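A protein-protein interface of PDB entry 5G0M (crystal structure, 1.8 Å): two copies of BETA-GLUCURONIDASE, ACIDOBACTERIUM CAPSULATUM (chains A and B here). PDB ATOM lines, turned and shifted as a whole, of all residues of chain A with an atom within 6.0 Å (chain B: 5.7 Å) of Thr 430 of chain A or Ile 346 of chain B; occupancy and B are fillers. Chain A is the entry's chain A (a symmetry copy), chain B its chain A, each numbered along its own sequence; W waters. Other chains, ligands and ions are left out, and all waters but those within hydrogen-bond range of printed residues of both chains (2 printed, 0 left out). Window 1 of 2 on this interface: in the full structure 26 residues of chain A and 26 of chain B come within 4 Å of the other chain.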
ATOM      1  N   ASP A 301     -24.366   6.585 -31.831  1.00  0.00           N
ATOM      2  CA  ASP A 301     -23.484   7.237 -30.867  1.00  0.00           C
ATOM      3  C   ASP A 301     -22.035   6.702 -30.827  1.00  0.00           C
ATOM      4  O   ASP A 301     -21.335   6.900 -29.814  1.00  0.00           O
ATOM      5  CB  ASP A 301     -24.113   7.199 -29.478  1.00  0.00           C
ATOM      6  CG  ASP A 301     -24.330   5.795 -28.924  1.00  0.00           C
ATOM      7  OD1 ASP A 301     -24.489   4.836 -29.714  1.00  0.00           O
ATOM      8  OD2 ASP A 301     -24.353   5.693 -27.695  1.00  0.00           O
ATOM      9  N   PHE A 303     -18.094   5.495 -32.874  1.00  0.00           N
ATOM     10  CA  PHE A 303     -17.113   5.858 -33.879  1.00  0.00           C
ATOM     11  C   PHE A 303     -17.522   5.476 -35.296  1.00  0.00           C
ATOM     12  O   PHE A 303     -17.215   6.223 -36.287  1.00  0.00           O
ATOM     13  CB  PHE A 303     -15.794   5.236 -33.523  1.00  0.00           C
ATOM     14  CG  PHE A 303     -14.738   5.557 -34.480  1.00  0.00           C
ATOM     15  CD1 PHE A 303     -14.299   6.884 -34.643  1.00  0.00           C
ATOM     16  CD2 PHE A 303     -14.212   4.570 -35.285  1.00  0.00           C
ATOM     17  CE1 PHE A 303     -13.282   7.163 -35.536  1.00  0.00           C
ATOM     18  CE2 PHE A 303     -13.218   4.862 -36.204  1.00  0.00           C
ATOM     19  CZ  PHE A 303     -12.750   6.168 -36.307  1.00  0.00           C
ATOM     20  N   PRO A 349     -18.940  11.288 -31.224  1.00  0.00           N
ATOM     21  CA  PRO A 349     -18.141  10.659 -32.235  1.00  0.00           C
ATOM     22  C   PRO A 349     -18.420  11.118 -33.700  1.00  0.00           C
ATOM     23  O   PRO A 349     -17.462  11.444 -34.459  1.00  0.00           O
ATOM     24  CB  PRO A 349     -18.398   9.177 -32.015  1.00  0.00           C
ATOM     25  CG  PRO A 349     -18.566   9.049 -30.573  1.00  0.00           C
ATOM     26  CD  PRO A 349     -19.374  10.307 -30.188  1.00  0.00           C
ATOM     27  N   ALA A 423     -10.476   5.310 -33.428  1.00  0.00           N
ATOM     28  CA  ALA A 423     -10.950   4.856 -32.148  1.00  0.00           C
ATOM     29  C   ALA A 423     -10.548   3.343 -31.995  1.00  0.00           C
ATOM     30  O   ALA A 423     -10.443   2.659 -32.977  1.00  0.00           O
ATOM     31  CB  ALA A 423     -12.462   4.976 -32.050  1.00  0.00           C
ATOM     32  N   PRO A 424     -10.418   2.849 -30.767  1.00  0.00           N
ATOM     33  CA  PRO A 424      -9.939   1.477 -30.588  1.00  0.00           C
ATOM     34  C   PRO A 424     -10.906   0.391 -31.014  1.00  0.00           C
ATOM     35  O   PRO A 424     -10.484  -0.742 -31.201  1.00  0.00           O
ATOM     36  CB  PRO A 424      -9.619   1.442 -29.079  1.00  0.00           C
ATOM     37  CG  PRO A 424     -10.564   2.416 -28.468  1.00  0.00           C
ATOM     38  CD  PRO A 424     -10.672   3.516 -29.468  1.00  0.00           C
ATOM     39  N   ASP A 428     -17.139   2.131 -30.165  1.00  0.00           N
ATOM     40  CA  ASP A 428     -16.783   2.906 -29.023  1.00  0.00           C
ATOM     41  C   ASP A 428     -17.607   4.173 -29.033  1.00  0.00           C
ATOM     42  O   ASP A 428     -17.775   4.815 -30.108  1.00  0.00           O
ATOM     43  CB  ASP A 428     -15.295   3.283 -29.100  1.00  0.00           C
ATOM     44  CG  ASP A 428     -14.676   3.545 -27.743  1.00  0.00           C
ATOM     45  OD1 ASP A 428     -15.393   3.970 -26.794  1.00  0.00           O
ATOM     46  OD2 ASP A 428     -13.433   3.369 -27.634  1.00  0.00           O
ATOM     47  N   THR A 429     -18.074   4.547 -27.870  1.00  0.00           N
ATOM     48  CA  THR A 429     -18.818   5.788 -27.673  1.00  0.00           C
ATOM     49  C   THR A 429     -17.945   7.022 -27.309  1.00  0.00           C
ATOM     50  O   THR A 429     -18.452   8.144 -27.110  1.00  0.00           O
ATOM     51  CB  THR A 429     -19.829   5.635 -26.551  1.00  0.00           C
ATOM     52  OG1 THR A 429     -19.141   5.274 -25.349  1.00  0.00           O
ATOM     53  CG2 THR A 429     -20.939   4.624 -26.895  1.00  0.00           C
ATOM     54  N   THR A 430     -16.651   6.754 -27.120  1.00  0.00           N
ATOM     55  CA  THR A 430     -15.726   7.743 -26.745  1.00  0.00           C
ATOM     56  C   THR A 430     -14.372   7.276 -27.331  1.00  0.00           C
ATOM     57  O   THR A 430     -14.351   6.461 -28.261  1.00  0.00           O
ATOM     58  CB  THR A 430     -15.725   7.963 -25.208  1.00  0.00           C
ATOM     59  OG1 THR A 430     -14.771   9.004 -24.879  1.00  0.00           O
ATOM     60  CG2 THR A 430     -15.359   6.697 -24.417  1.00  0.00           C
ATOM     61  N   ASP A 431     -13.272   7.808 -26.805  1.00  0.00           N
ATOM     62  CA  ASP A 431     -11.923   7.508 -27.269  1.00  0.00           C
ATOM     63  C   ASP A 431     -11.663   7.869 -28.742  1.00  0.00           C
ATOM     64  O   ASP A 431     -10.883   7.164 -29.435  1.00  0.00           O
ATOM     65  CB  ASP A 431     -11.612   6.028 -27.090  1.00  0.00           C
ATOM     66  CG  ASP A 431     -11.779   5.528 -25.650  1.00  0.00           C
ATOM     67  OD1 ASP A 431     -11.570   6.315 -24.689  1.00  0.00           O
ATOM     68  OD2 ASP A 431     -12.156   4.330 -25.497  1.00  0.00           O
ATOM     69  N   VAL A 432     -12.372   8.867 -29.288  1.00  0.00           N
ATOM     70  CA  VAL A 432     -12.270   9.180 -30.698  1.00  0.00           C
ATOM     71  C   VAL A 432     -11.259  10.317 -30.865  1.00  0.00           C
ATOM     72  O   VAL A 432     -11.360  11.366 -30.224  1.00  0.00           O
ATOM     73  CB  VAL A 432     -13.632   9.563 -31.353  1.00  0.00           C
ATOM     74  CG1 VAL A 432     -13.469   9.928 -32.815  1.00  0.00           C
ATOM     75  CG2 VAL A 432     -14.635   8.405 -31.262  1.00  0.00           C
ATOM     76  N   THR A 433     -10.304  10.141 -31.769  1.00  0.00           N
ATOM     77  CA  THR A 433      -9.366  11.208 -32.035  1.00  0.00           C
ATOM     78  C   THR A 433      -9.228  11.495 -33.528  1.00  0.00           C
ATOM     79  O   THR A 433      -9.473  10.650 -34.375  1.00  0.00           O
ATOM     80  CB  THR A 433      -7.971  10.909 -31.400  1.00  0.00           C
ATOM     81  OG1 THR A 433      -7.449   9.728 -31.964  1.00  0.00           O
ATOM     82  CG2 THR A 433      -8.105  10.774 -29.896  1.00  0.00           C
ATOM     83  N   PRO A 438      -8.186  14.681 -29.224  1.00  0.00           N
ATOM     84  CA  PRO A 438      -9.625  14.978 -29.090  1.00  0.00           C
ATOM     85  C   PRO A 438      -9.908  16.467 -29.351  1.00  0.00           C
ATOM     86  O   PRO A 438      -8.983  17.315 -29.306  1.00  0.00           O
ATOM     87  CB  PRO A 438      -9.896  14.640 -27.611  1.00  0.00           C
ATOM     88  CG  PRO A 438      -8.583  15.102 -26.931  1.00  0.00           C
ATOM     89  CD  PRO A 438      -7.517  14.646 -27.898  1.00  0.00           C
ATOM     90  N   PHE B  65      -2.304  15.449 -18.771  1.00  0.00           N
ATOM     91  CA  PHE B  65      -3.394  14.871 -17.987  1.00  0.00           C
ATOM     92  C   PHE B  65      -2.968  14.682 -16.502  1.00  0.00           C
ATOM     93  O   PHE B  65      -3.747  14.973 -15.617  1.00  0.00           O
ATOM     94  CB  PHE B  65      -3.876  13.565 -18.617  1.00  0.00           C
ATOM     95  CG  PHE B  65      -4.765  13.755 -19.830  1.00  0.00           C
ATOM     96  CD1 PHE B  65      -6.090  14.131 -19.662  1.00  0.00           C
ATOM     97  CD2 PHE B  65      -4.261  13.586 -21.110  1.00  0.00           C
ATOM     98  CE1 PHE B  65      -6.892  14.365 -20.777  1.00  0.00           C
ATOM     99  CE2 PHE B  65      -5.057  13.771 -22.233  1.00  0.00           C
ATOM    100  CZ  PHE B  65      -6.385  14.187 -22.043  1.00  0.00           C
ATOM    101  N   PRO B 336      -8.786   6.157 -15.679  1.00  0.00           N
ATOM    102  CA  PRO B 336      -9.032   7.582 -15.666  1.00  0.00           C
ATOM    103  C   PRO B 336      -8.677   8.230 -17.002  1.00  0.00           C
ATOM    104  O   PRO B 336      -9.441   9.068 -17.542  1.00  0.00           O
ATOM    105  CB  PRO B 336      -8.121   8.071 -14.526  1.00  0.00           C
ATOM    106  CG  PRO B 336      -7.971   6.929 -13.655  1.00  0.00           C
ATOM    107  CD  PRO B 336      -7.932   5.744 -14.538  1.00  0.00           C
ATOM    108  N   VAL B 337      -7.495   7.891 -17.515  1.00  0.00           N
ATOM    109  CA  VAL B 337      -7.030   8.363 -18.820  1.00  0.00           C
ATOM    110  C   VAL B 337      -6.870   7.203 -19.758  1.00  0.00           C
ATOM    111  O   VAL B 337      -6.189   6.211 -19.449  1.00  0.00           O
ATOM    112  CB  VAL B 337      -5.703   9.140 -18.738  1.00  0.00           C
ATOM    113  CG1 VAL B 337      -5.366   9.758 -20.113  1.00  0.00           C
ATOM    114  CG2 VAL B 337      -5.814  10.186 -17.619  1.00  0.00           C
ATOM    115  N   ALA B 338      -7.491   7.362 -20.949  1.00  0.00           N
ATOM    116  CA  ALA B 338      -7.368   6.405 -22.054  1.00  0.00           C
ATOM    117  C   ALA B 338      -6.547   6.899 -23.244  1.00  0.00           C
ATOM    118  O   ALA B 338      -6.460   8.099 -23.534  1.00  0.00           O
ATOM    119  CB  ALA B 338      -8.748   5.936 -22.528  1.00  0.00           C
ATOM    120  N   GLY B 339      -5.943   5.962 -23.934  1.00  0.00           N
ATOM    121  CA  GLY B 339      -5.203   6.263 -25.179  1.00  0.00           C
ATOM    122  C   GLY B 339      -3.819   5.675 -25.445  1.00  0.00           C
ATOM    123  O   GLY B 339      -3.368   4.812 -24.730  1.00  0.00           O
ATOM    124  N   GLY B 344      -3.238   9.433 -29.414  1.00  0.00           N
ATOM    125  CA  GLY B 344      -3.681  10.426 -28.436  1.00  0.00           C
ATOM    126  C   GLY B 344      -4.462   9.907 -27.228  1.00  0.00           C
ATOM    127  O   GLY B 344      -4.829   8.768 -27.183  1.00  0.00           O
ATOM    128  N   PHE B 345      -4.645  10.793 -26.248  1.00  0.00           N
ATOM    129  CA  PHE B 345      -5.161  10.464 -24.960  1.00  0.00           C
ATOM    130  C   PHE B 345      -6.403  11.304 -24.680  1.00  0.00           C
ATOM    131  O   PHE B 345      -6.492  12.429 -25.164  1.00  0.00           O
ATOM    132  CB  PHE B 345      -4.135  10.684 -23.837  1.00  0.00           C
ATOM    133  CG  PHE B 345      -2.988   9.716 -23.878  1.00  0.00           C
ATOM    134  CD1 PHE B 345      -1.906   9.954 -24.664  1.00  0.00           C
ATOM    135  CD2 PHE B 345      -3.007   8.541 -23.134  1.00  0.00           C
ATOM    136  CE1 PHE B 345      -0.839   9.062 -24.727  1.00  0.00           C
ATOM    137  CE2 PHE B 345      -1.955   7.649 -23.190  1.00  0.00           C
ATOM    138  CZ  PHE B 345      -0.853   7.906 -23.979  1.00  0.00           C
ATOM    139  N   ILE B 346      -7.348  10.735 -23.916  1.00  0.00           N
ATOM    140  CA  ILE B 346      -8.564  11.467 -23.475  1.00  0.00           C
ATOM    141  C   ILE B 346      -8.924  11.172 -22.056  1.00  0.00           C
ATOM    142  O   ILE B 346      -8.583  10.077 -21.543  1.00  0.00           O
ATOM    143  CB  ILE B 346      -9.803  11.079 -24.295  1.00  0.00           C
ATOM    144  CG1 ILE B 346     -10.247   9.678 -23.971  1.00  0.00           C
ATOM    145  CG2 ILE B 346      -9.536  11.148 -25.802  1.00  0.00           C
ATOM    146  CD1 ILE B 346     -11.744   9.630 -23.834  1.00  0.00           C
ATOM    147  N   ALA B 347      -9.680  12.093 -21.440  1.00  0.00           N
ATOM    148  CA  ALA B 347     -10.158  11.901 -20.111  1.00  0.00           C
ATOM    149  C   ALA B 347     -11.454  11.091 -20.153  1.00  0.00           C
ATOM    150  O   ALA B 347     -12.459  11.539 -20.730  1.00  0.00           O
ATOM    151  CB  ALA B 347     -10.406  13.230 -19.370  1.00  0.00           C
ATOM    152  N   ARG B 348     -11.453   9.973 -19.461  1.00  0.00           N
ATOM    153  CA  ARG B 348     -12.678   9.178 -19.286  1.00  0.00           C
ATOM    154  C   ARG B 348     -13.525   9.777 -18.126  1.00  0.00           C
ATOM    155  O   ARG B 348     -13.056  10.681 -17.380  1.00  0.00           O
ATOM    156  CB  ARG B 348     -12.298   7.720 -18.990  1.00  0.00           C
ATOM    157  CG  ARG B 348     -11.721   6.953 -20.152  1.00  0.00           C
ATOM    158  CD  ARG B 348     -12.860   6.530 -21.097  1.00  0.00           C
ATOM    159  NE  ARG B 348     -12.403   5.505 -22.033  1.00  0.00           N
ATOM    160  CZ  ARG B 348     -12.152   4.221 -21.773  1.00  0.00           C
ATOM    161  NH1 ARG B 348     -12.335   3.673 -20.573  1.00  0.00           N
ATOM    162  NH2 ARG B 348     -11.695   3.458 -22.739  1.00  0.00           N
ATOM    163  N   THR B 429     -21.505   7.256 -20.787  1.00  0.00           N
ATOM    164  CA  THR B 429     -20.087   7.020 -21.041  1.00  0.00           C
ATOM    165  C   THR B 429     -19.298   8.261 -21.547  1.00  0.00           C
ATOM    166  O   THR B 429     -18.080   8.198 -21.807  1.00  0.00           O
ATOM    167  CB  THR B 429     -19.903   5.940 -22.093  1.00  0.00           C
ATOM    168  OG1 THR B 429     -20.562   6.345 -23.298  1.00  0.00           O
ATOM    169  CG2 THR B 429     -20.398   4.563 -21.613  1.00  0.00           C
ATOM    170  N   THR B 430     -20.047   9.340 -21.783  1.00  0.00           N
ATOM    171  CA  THR B 430     -19.506  10.536 -22.283  1.00  0.00           C
ATOM    172  C   THR B 430     -20.420  11.658 -21.734  1.00  0.00           C
ATOM    173  O   THR B 430     -21.132  11.444 -20.746  1.00  0.00           O
ATOM    174  CB  THR B 430     -19.384  10.499 -23.830  1.00  0.00           C
ATOM    175  OG1 THR B 430     -18.802  11.745 -24.290  1.00  0.00           O
ATOM    176  CG2 THR B 430     -20.734  10.299 -24.537  1.00  0.00           C
ATOM    177  N   GLY B 440     -10.020  18.977 -22.410  1.00  0.00           N
ATOM    178  CA  GLY B 440      -9.547  18.891 -23.756  1.00  0.00           C
ATOM    179  C   GLY B 440      -8.297  18.048 -23.995  1.00  0.00           C
ATOM    180  O   GLY B 440      -7.993  17.106 -23.207  1.00  0.00           O
HETATM  181  O   HOH W   1     -15.709   9.615 -22.295  1.00  0.00           O
HETATM  182  O   HOH W   2     -18.018  10.904 -26.860  1.00  0.00           O
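N of Thr 430 of chain A is in hydrogen-bond range of OD1 of Asp 428 of chain A, at 3.1 Å. The side-chain carboxylate (OD2) of Asp 431 of chain A lies close to the side-chain carboxylate (OD2) of Asp 428 of chain A, 2.7 Å away. The backbone NH (N) of Arg 348 of chain B is in hydrogen-bond range of the backbone carbonyl oxygen (O) of Pro 336 of chain B, 2.9 Å away. N of Ile 346 of chain B sits at hydrogen-bond distance from O of Ala 338 of chain B (2.8 Å).
The guanidinium group (NE) of Arg 348 of chain B lies within salt-bridge range of the side-chain carboxylate (OD1) of Asp 431 of chain A (2.9 Å). The side-chain hydroxyl of Thr 429 of chain B sits at hydrogen-bond distance from the side-chain hydroxyl of Thr 429 of chain A (2.7 Å).
Thr 430 of chain A touches Ile 346 of chain B (OG1 to CD1, 3.3 Å). Thr 430 of chain A touches Arg 348 of chain B (CG2 to NE, 3.98 Å). Ala 338 of chain B touches Asp 431 of chain A (CB to OD1, 3.6 Å). Asp 431 of chain A touches Ile 346 of chain B (OD1 to CD1, 3.4 Å). CD of Pro 438 of chain A touches O of Phe 345 of chain B, 3.7 Å away. Ile 346 of chain B touches Pro 438 of chain A (CG2 to CB, 3.9 Å).
Thr 429 of chain B touches its own counterpart, Thr 429 of chain A. Positions printed for both chains: 429 and 430.
Of the 12 printed residues of chain A, 4 touch a printed residue of chain B. Hydrophobic or aromatic side chains of chain A that line the printed part of chain B: Pro 438. Along chain A the printed residues that touch a printed residue of chain B span positions 429 to 438. Of the 13 printed residues of chain B, 5 touch a printed residue of chain A. Printed residues of chain B that touch a printed residue of chain A: Ala 338, Phe 345, Ile 346, Arg 348 and Thr 429. Among the printed residues, Asp or Glu carboxylates within 4 Å of a Lys or Arg side-chain nitrogen of the other chain: Asp 431 of chain A with Arg 348 of chain B (2.9 Å).
Printed residues of chain B within 4 Å of Thr 430 of chain A: Ile 346 and Arg 348. Of the printed residues of chain A, Ala 338 of chain B touches Asp 431 (3.6 Å). Of the printed residues of chain B, Thr 429 of chain A touches Thr 429 (2.7 Å). Printed residues of chain A within 4 Å of Phe 345 of chain B: Pro 438 (3.7 Å). Printed residues of chain B within 4 Å of Pro 438 of chain A: Phe 345 and Ile 346. Of the printed residues of chain A, Arg 348 of chain B touches Thr 430 and Asp 431. Phe 65 of chain B touches none of the printed residues of chain A. Val 337 of chain B touches none of the printed residues of chain A. The nearest printed residue of chain B that does not touch Thr 429 of chain A is Thr 430 of chain B (4.1 Å).
Water W1 bridges the backbone carbonyl oxygen of Thr 429 of chain B (2.8 Å) and the side-chain hydroxyl of Thr 430 of chain A (2.8 Å). Water W2 bridges the backbone carbonyl oxygen (O) of Thr 429 of chain A and the side-chain hydroxyl (OG1) of Thr 430 of chain B.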
